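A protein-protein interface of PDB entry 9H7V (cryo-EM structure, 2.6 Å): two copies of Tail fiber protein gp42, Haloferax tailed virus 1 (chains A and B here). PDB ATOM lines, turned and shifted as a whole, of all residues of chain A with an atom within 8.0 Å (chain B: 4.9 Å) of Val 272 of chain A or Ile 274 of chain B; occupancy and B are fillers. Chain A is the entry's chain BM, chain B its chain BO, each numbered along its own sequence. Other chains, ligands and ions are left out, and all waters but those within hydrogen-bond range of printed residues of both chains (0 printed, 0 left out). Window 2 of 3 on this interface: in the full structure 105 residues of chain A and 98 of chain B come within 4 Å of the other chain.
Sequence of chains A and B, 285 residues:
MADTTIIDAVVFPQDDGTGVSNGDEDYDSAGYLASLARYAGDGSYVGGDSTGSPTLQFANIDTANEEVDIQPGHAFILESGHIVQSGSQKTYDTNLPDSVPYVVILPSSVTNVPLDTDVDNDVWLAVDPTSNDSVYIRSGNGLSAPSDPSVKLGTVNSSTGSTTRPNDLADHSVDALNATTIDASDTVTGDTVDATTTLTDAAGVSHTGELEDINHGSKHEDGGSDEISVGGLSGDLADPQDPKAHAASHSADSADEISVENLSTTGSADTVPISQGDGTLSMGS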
ATOM      1  N   VAL A 260      11.900  -7.312  36.518  1.00  0.00           N
ATOM      2  CA  VAL A 260      10.996  -7.748  35.460  1.00  0.00           C
ATOM      3  C   VAL A 260      10.164  -8.949  35.921  1.00  0.00           C
ATOM      4  O   VAL A 260       8.986  -9.041  35.578  1.00  0.00           O
ATOM      5  CB  VAL A 260      11.718  -7.985  34.114  1.00  0.00           C
ATOM      6  CG1 VAL A 260      10.828  -8.666  33.082  1.00  0.00           C
ATOM      7  CG2 VAL A 260      12.239  -6.678  33.544  1.00  0.00           C
ATOM      8  N   GLU A 261      10.763  -9.827  36.740  1.00  0.00           N
ATOM      9  CA  GLU A 261      10.101 -11.030  37.231  1.00  0.00           C
ATOM     10  C   GLU A 261       8.987 -10.703  38.234  1.00  0.00           C
ATOM     11  O   GLU A 261       8.265 -11.605  38.657  1.00  0.00           O
ATOM     12  CB  GLU A 261      11.113 -12.054  37.762  1.00  0.00           C
ATOM     13  CG  GLU A 261      12.047 -11.524  38.841  1.00  0.00           C
ATOM     14  CD  GLU A 261      13.374 -10.959  38.358  1.00  0.00           C
ATOM     15  OE1 GLU A 261      13.416 -10.376  37.254  1.00  0.00           O
ATOM     16  OE2 GLU A 261      14.367 -11.099  39.095  1.00  0.00           O
ATOM     17  N   THR A 265       1.990  -9.980  33.168  1.00  0.00           N
ATOM     18  CA  THR A 265       1.844 -10.238  31.739  1.00  0.00           C
ATOM     19  C   THR A 265       0.536 -10.979  31.459  1.00  0.00           C
ATOM     20  O   THR A 265       0.064 -11.760  32.286  1.00  0.00           O
ATOM     21  CB  THR A 265       3.052 -10.955  31.111  1.00  0.00           C
ATOM     22  OG1 THR A 265       2.863 -10.956  29.694  1.00  0.00           O
ATOM     23  CG2 THR A 265       3.250 -12.375  31.600  1.00  0.00           C
ATOM     24  N   GLY A 267       0.546 -12.707  28.582  1.00  0.00           N
ATOM     25  CA  GLY A 267       1.088 -13.774  27.751  1.00  0.00           C
ATOM     26  C   GLY A 267       0.962 -15.146  28.415  1.00  0.00           C
ATOM     27  O   GLY A 267       1.224 -15.281  29.609  1.00  0.00           O
ATOM     28  N   SER A 268       0.559 -16.149  27.619  1.00  0.00           N
ATOM     29  CA  SER A 268       0.372 -17.525  28.063  1.00  0.00           C
ATOM     30  C   SER A 268       1.714 -18.158  28.439  1.00  0.00           C
ATOM     31  O   SER A 268       2.761 -17.542  28.252  1.00  0.00           O
ATOM     32  CB  SER A 268      -0.359 -18.330  27.012  1.00  0.00           C
ATOM     33  OG  SER A 268      -1.615 -17.741  26.704  1.00  0.00           O
ATOM     34  N   ALA A 269       1.676 -19.390  28.972  1.00  0.00           N
ATOM     35  CA  ALA A 269       2.861 -20.092  29.449  1.00  0.00           C
ATOM     36  C   ALA A 269       3.885 -20.262  28.325  1.00  0.00           C
ATOM     37  O   ALA A 269       3.514 -20.511  27.178  1.00  0.00           O
ATOM     38  CB  ALA A 269       2.468 -21.422  30.047  1.00  0.00           C
ATOM     39  N   ASP A 270       5.168 -20.093  28.683  1.00  0.00           N
ATOM     40  CA  ASP A 270       6.344 -20.250  27.828  1.00  0.00           C
ATOM     41  C   ASP A 270       6.523 -19.088  26.842  1.00  0.00           C
ATOM     42  O   ASP A 270       7.415 -19.153  25.994  1.00  0.00           O
ATOM     43  CB  ASP A 270       6.437 -21.640  27.174  1.00  0.00           C
ATOM     44  CG  ASP A 270       6.583 -22.812  28.134  1.00  0.00           C
ATOM     45  OD1 ASP A 270       7.075 -22.603  29.264  1.00  0.00           O
ATOM     46  OD2 ASP A 270       6.207 -23.935  27.739  1.00  0.00           O
ATOM     47  N   THR A 271       5.720 -18.015  26.960  1.00  0.00           N
ATOM     48  CA  THR A 271       5.861 -16.870  26.064  1.00  0.00           C
ATOM     49  C   THR A 271       6.998 -15.952  26.518  1.00  0.00           C
ATOM     50  O   THR A 271       7.283 -15.850  27.710  1.00  0.00           O
ATOM     51  CB  THR A 271       4.556 -16.088  25.845  1.00  0.00           C
ATOM     52  OG1 THR A 271       4.040 -15.655  27.104  1.00  0.00           O
ATOM     53  CG2 THR A 271       3.512 -16.864  25.070  1.00  0.00           C
ATOM     54  N   VAL A 272       7.617 -15.278  25.536  1.00  0.00           N
ATOM     55  CA  VAL A 272       8.772 -14.403  25.701  1.00  0.00           C
ATOM     56  C   VAL A 272       8.381 -13.000  25.225  1.00  0.00           C
ATOM     57  O   VAL A 272       7.710 -12.872  24.200  1.00  0.00           O
ATOM     58  CB  VAL A 272       9.986 -14.931  24.903  1.00  0.00           C
ATOM     59  CG1 VAL A 272      11.260 -14.146  25.177  1.00  0.00           C
ATOM     60  CG2 VAL A 272      10.230 -16.421  25.107  1.00  0.00           C
ATOM     61  N   PRO A 273       8.768 -11.909  25.936  1.00  0.00           N
ATOM     62  CA  PRO A 273       8.606 -10.551  25.409  1.00  0.00           C
ATOM     63  C   PRO A 273       9.649 -10.267  24.330  1.00  0.00           C
ATOM     64  O   PRO A 273      10.850 -10.369  24.581  1.00  0.00           O
ATOM     65  CB  PRO A 273       8.793  -9.647  26.637  1.00  0.00           C
ATOM     66  CG  PRO A 273       9.655 -10.456  27.587  1.00  0.00           C
ATOM     67  CD  PRO A 273       9.340 -11.909  27.292  1.00  0.00           C
ATOM     68  N   ILE A 274       9.173  -9.945  23.120  1.00  0.00           N
ATOM     69  CA  ILE A 274      10.037  -9.773  21.960  1.00  0.00           C
ATOM     70  C   ILE A 274       9.700  -8.458  21.257  1.00  0.00           C
ATOM     71  O   ILE A 274       8.543  -8.036  21.235  1.00  0.00           O
ATOM     72  CB  ILE A 274       9.987 -10.994  21.007  1.00  0.00           C
ATOM     73  CG1 ILE A 274       8.587 -11.250  20.432  1.00  0.00           C
ATOM     74  CG2 ILE A 274      10.585 -12.233  21.664  1.00  0.00           C
ATOM     75  CD1 ILE A 274       8.553 -12.193  19.245  1.00  0.00           C
ATOM     76  N   SER A 275      10.734  -7.824  20.689  1.00  0.00           N
ATOM     77  CA  SER A 275      10.607  -6.551  19.996  1.00  0.00           C
ATOM     78  C   SER A 275      10.049  -6.768  18.591  1.00  0.00           C
ATOM     79  O   SER A 275      10.425  -7.720  17.907  1.00  0.00           O
ATOM     80  CB  SER A 275      11.927  -5.828  19.957  1.00  0.00           C
ATOM     81  OG  SER A 275      11.816  -4.594  19.261  1.00  0.00           O
ATOM     82  N   LEU A 281       7.171  -3.634  22.112  1.00  0.00           N
ATOM     83  CA  LEU A 281       7.279  -4.997  22.617  1.00  0.00           C
ATOM     84  C   LEU A 281       5.976  -5.762  22.375  1.00  0.00           C
ATOM     85  O   LEU A 281       4.919  -5.159  22.182  1.00  0.00           O
ATOM     86  CB  LEU A 281       7.632  -4.964  24.110  1.00  0.00           C
ATOM     87  CG  LEU A 281       9.093  -4.670  24.451  1.00  0.00           C
ATOM     88  CD1 LEU A 281       9.258  -4.499  25.949  1.00  0.00           C
ATOM     89  CD2 LEU A 281      10.010  -5.777  23.947  1.00  0.00           C
ATOM     90  N   SER A 282       6.084  -7.101  22.396  1.00  0.00           N
ATOM     91  CA  SER A 282       4.998  -8.048  22.173  1.00  0.00           C
ATOM     92  C   SER A 282       5.307  -9.350  22.916  1.00  0.00           C
ATOM     93  O   SER A 282       6.452  -9.570  23.302  1.00  0.00           O
ATOM     94  CB  SER A 282       4.814  -8.302  20.695  1.00  0.00           C
ATOM     95  OG  SER A 282       5.976  -8.904  20.136  1.00  0.00           O
ATOM     96  N   MET A 283       4.295 -10.213  23.099  1.00  0.00           N
ATOM     97  CA  MET A 283       4.501 -11.534  23.681  1.00  0.00           C
ATOM     98  C   MET A 283       4.349 -12.610  22.604  1.00  0.00           C
ATOM     99  O   MET A 283       3.327 -12.663  21.921  1.00  0.00           O
ATOM    100  CB  MET A 283       3.527 -11.799  24.835  1.00  0.00           C
ATOM    101  CG  MET A 283       4.097 -11.465  26.203  1.00  0.00           C
ATOM    102  SD  MET A 283       5.289 -12.702  26.783  1.00  0.00           S
ATOM    103  CE  MET A 283       5.751 -12.003  28.365  1.00  0.00           C
ATOM    104  N   GLY A 284       5.382 -13.460  22.462  1.00  0.00           N
ATOM    105  CA  GLY A 284       5.450 -14.515  21.454  1.00  0.00           C
ATOM    106  C   GLY A 284       6.213 -15.750  21.939  1.00  0.00           C
ATOM    107  O   GLY A 284       6.599 -15.812  23.104  1.00  0.00           O
ATOM    108  N   SER A 285       6.447 -16.719  21.037  1.00  0.00           N
ATOM    109  CA  SER A 285       7.015 -18.015  21.396  1.00  0.00           C
ATOM    110  C   SER A 285       8.378 -18.241  20.735  1.00  0.00           C
ATOM    111  O   SER A 285       8.555 -17.927  19.558  1.00  0.00           O
ATOM    112  CB  SER A 285       6.057 -19.136  21.063  1.00  0.00           C
ATOM    113  OG  SER A 285       4.857 -19.019  21.813  1.00  0.00           O
ATOM    114  N   VAL B 272      16.427 -15.023  30.642  1.00  0.00           N
ATOM    115  CA  VAL B 272      15.422 -14.356  29.823  1.00  0.00           C
ATOM    116  C   VAL B 272      14.117 -14.286  30.623  1.00  0.00           C
ATOM    117  O   VAL B 272      13.762 -15.265  31.279  1.00  0.00           O
ATOM    118  CB  VAL B 272      15.215 -15.111  28.489  1.00  0.00           C
ATOM    119  CG1 VAL B 272      14.191 -14.443  27.581  1.00  0.00           C
ATOM    120  CG2 VAL B 272      16.513 -15.354  27.731  1.00  0.00           C
ATOM    121  N   PRO B 273      13.358 -13.156  30.615  1.00  0.00           N
ATOM    122  CA  PRO B 273      12.011 -13.142  31.193  1.00  0.00           C
ATOM    123  C   PRO B 273      11.018 -13.919  30.330  1.00  0.00           C
ATOM    124  O   PRO B 273      10.873 -13.629  29.145  1.00  0.00           O
ATOM    125  CB  PRO B 273      11.639 -11.652  31.260  1.00  0.00           C
ATOM    126  CG  PRO B 273      12.496 -10.990  30.199  1.00  0.00           C
ATOM    127  CD  PRO B 273      13.756 -11.829  30.109  1.00  0.00           C
ATOM    128  N   ILE B 274      10.374 -14.933  30.928  1.00  0.00           N
ATOM    129  CA  ILE B 274       9.382 -15.755  30.244  1.00  0.00           C
ATOM    130  C   ILE B 274       8.170 -15.964  31.155  1.00  0.00           C
ATOM    131  O   ILE B 274       8.307 -16.005  32.378  1.00  0.00           O
ATOM    132  CB  ILE B 274       9.969 -17.089  29.714  1.00  0.00           C
ATOM    133  CG1 ILE B 274      10.357 -18.064  30.832  1.00  0.00           C
ATOM    134  CG2 ILE B 274      11.113 -16.862  28.730  1.00  0.00           C
ATOM    135  CD1 ILE B 274      10.353 -19.525  30.424  1.00  0.00           C
ATOM    136  N   SER B 275       6.987 -16.101  30.538  1.00  0.00           N
ATOM    137  CA  SER B 275       5.728 -16.256  31.256  1.00  0.00           C
ATOM    138  C   SER B 275       5.548 -17.697  31.733  1.00  0.00           C
ATOM    139  O   SER B 275       5.847 -18.642  31.004  1.00  0.00           O
ATOM    140  CB  SER B 275       4.557 -15.805  30.418  1.00  0.00           C
ATOM    141  OG  SER B 275       3.328 -16.021  31.100  1.00  0.00           O
ATOM    142  N   GLN B 276       5.036 -17.827  32.964  1.00  0.00           N
ATOM    143  CA  GLN B 276       4.678 -19.100  33.572  1.00  0.00           C
ATOM    144  C   GLN B 276       3.196 -19.398  33.339  1.00  0.00           C
ATOM    145  O   GLN B 276       2.711 -20.464  33.724  1.00  0.00           O
ATOM    146  CB  GLN B 276       4.943 -19.057  35.081  1.00  0.00           C
ATOM    147  CG  GLN B 276       6.418 -19.074  35.466  1.00  0.00           C
ATOM    148  CD  GLN B 276       7.091 -20.413  35.270  1.00  0.00           C
ATOM    149  OE1 GLN B 276       6.504 -21.470  35.493  1.00  0.00           O
ATOM    150  NE2 GLN B 276       8.347 -20.376  34.855  1.00  0.00           N
ATOM    151  N   THR B 280       2.139 -14.460  35.531  1.00  0.00           N
ATOM    152  CA  THR B 280       3.409 -14.425  36.250  1.00  0.00           C
ATOM    153  C   THR B 280       4.600 -14.582  35.299  1.00  0.00           C
ATOM    154  O   THR B 280       4.604 -15.480  34.457  1.00  0.00           O
ATOM    155  CB  THR B 280       3.414 -15.493  37.354  1.00  0.00           C
ATOM    156  OG1 THR B 280       2.302 -15.255  38.218  1.00  0.00           O
ATOM    157  CG2 THR B 280       4.688 -15.528  38.173  1.00  0.00           C
ATOM    158  N   LEU B 281       5.617 -13.722  35.472  1.00  0.00           N
ATOM    159  CA  LEU B 281       6.878 -13.803  34.745  1.00  0.00           C
ATOM    160  C   LEU B 281       7.925 -14.546  35.578  1.00  0.00           C
ATOM    161  O   LEU B 281       7.775 -14.682  36.792  1.00  0.00           O
ATOM    162  CB  LEU B 281       7.354 -12.392  34.384  1.00  0.00           C
ATOM    163  CG  LEU B 281       6.612 -11.713  33.232  1.00  0.00           C
ATOM    164  CD1 LEU B 281       6.841 -10.214  33.261  1.00  0.00           C
ATOM    165  CD2 LEU B 281       7.031 -12.293  31.886  1.00  0.00           C
ATOM    166  N   SER B 282       8.985 -15.019  34.899  1.00  0.00           N
ATOM    167  CA  SER B 282      10.054 -15.816  35.490  1.00  0.00           C
ATOM    168  C   SER B 282      11.338 -15.669  34.676  1.00  0.00           C
ATOM    169  O   SER B 282      11.285 -15.370  33.485  1.00  0.00           O
ATOM    170  CB  SER B 282       9.648 -17.269  35.583  1.00  0.00           C
ATOM    171  OG  SER B 282       9.358 -17.801  34.297  1.00  0.00           O
ATOM    172  N   GLY B 284      13.787 -17.602  32.848  1.00  0.00           N
ATOM    173  CA  GLY B 284      14.134 -18.845  32.178  1.00  0.00           C
ATOM    174  C   GLY B 284      15.505 -18.753  31.513  1.00  0.00           C
ATOM    175  O   GLY B 284      16.145 -17.702  31.548  1.00  0.00           O
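Of the 17 printed residues of chain A, 11 touch a printed residue of chain B. Among the printed residues, 16 pairs touch across the chains.
Pro 273 of chain B touches Val 260 of chain A. Val 260 of chain A touches Leu 281 of chain B (O to CD1, 3.4 Å). Glu 261 of chain A touches Leu 281 of chain B (O to O, 3.6 Å). Leu 281 of chain B touches Thr 265 of chain A (CD2 to CG2, 3.8 Å). Gln 276 of chain B touches Ala 269 of chain A. O of Thr 271 of chain A touches CA of Ile 274 of chain B (3.3 Å). Val 272 of chain B touches Val 272 of chain A (CG1 to CG1, 3.8 Å). Ile 274 of chain B touches Val 272 of chain A. Pro 273 of chain A touches Pro 273 of chain B. Met 283 of chain A touches Leu 281 of chain B.
N of Val 272 of chain A sits close to SD of Met 283 of chain A. The side-chain amide nitrogen (NE2) of Gln 276 of chain B is in hydrogen-bond range of the side-chain hydroxyl (OG) of Ser 282 of chain B (2.8 Å). The backbone NH (N) of Gly 284 of chain B lies within hydrogen-bond range of the backbone carbonyl oxygen (O) of Val 272 of chain B, 2.8 Å away. OG1 of Thr 265 of chain A is in hydrogen-bond range of N of Gly 267 of chain A, 3.1 Å away. The backbone carbonyl oxygen (O) of Ser 268 of chain A sits at hydrogen-bond distance from the side-chain hydroxyl (OG1) of Thr 271 of chain A, 2.6 Å away. The backbone NH (N) of Ile 274 of chain B sits at hydrogen-bond distance from the backbone carbonyl oxygen (O) of Ser 282 of chain B, at 2.7 Å.
Val 272 of chain A touches its own counterpart, Val 272 of chain B. Val 272 of chain A touches Ile 274 of chain B, but with the chains exchanged Ile 274 of chain A does not touch Val 272 of chain B (7.3 Å). Pro 273 of chain A touches its own counterpart, Pro 273 of chain B. Positions printed for both chains: 272, 273, 274, 275, 281, 282 and 284. Of the 16 pairs that touch across the chains among the printed residues, 2 have their exchanged pair printed and touching as well.
The backbone carbonyl oxygen (O) of Ser 268 of chain A sits at hydrogen-bond distance from the side-chain hydroxyl (OG) of Ser 275 of chain B. The backbone carbonyl oxygen (O) of Gly 267 of chain A lies within hydrogen-bond range of the side-chain hydroxyl (OG) of Ser 275 of chain B (2.7 Å). The backbone NH (N) of Asp 270 of chain A sits at hydrogen-bond distance from the backbone carbonyl oxygen (O) of Ser 275 of chain B. O of Thr 271 of chain A lies within hydrogen-bond range of N of Ser 275 of chain B (2.9 Å).
Ile 274 of chain B touches just these residues of chain A: Thr 271 and Val 272. Of the printed residues of chain B, Pro 273 of chain A touches Pro 273 (3.0 Å). Printed residues of chain B within 4 Å of Thr 265 of chain A: Ser 275 and Leu 281. Printed residues of chain A within 4 Å of Pro 273 of chain B: Val 260 (3.6 Å) and Pro 273 (3.0 Å). Of the printed residues of chain A, Gln 276 of chain B touches Ala 269 (3.8 Å). Ser 285 of chain A touches none of the printed residues of chain B. Thr 280 of chain B touches none of the printed residues of chain A. The nearest residue of chain A that does not touch Ile 274 of chain B is Asp 270 of chain A (4.6 Å).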
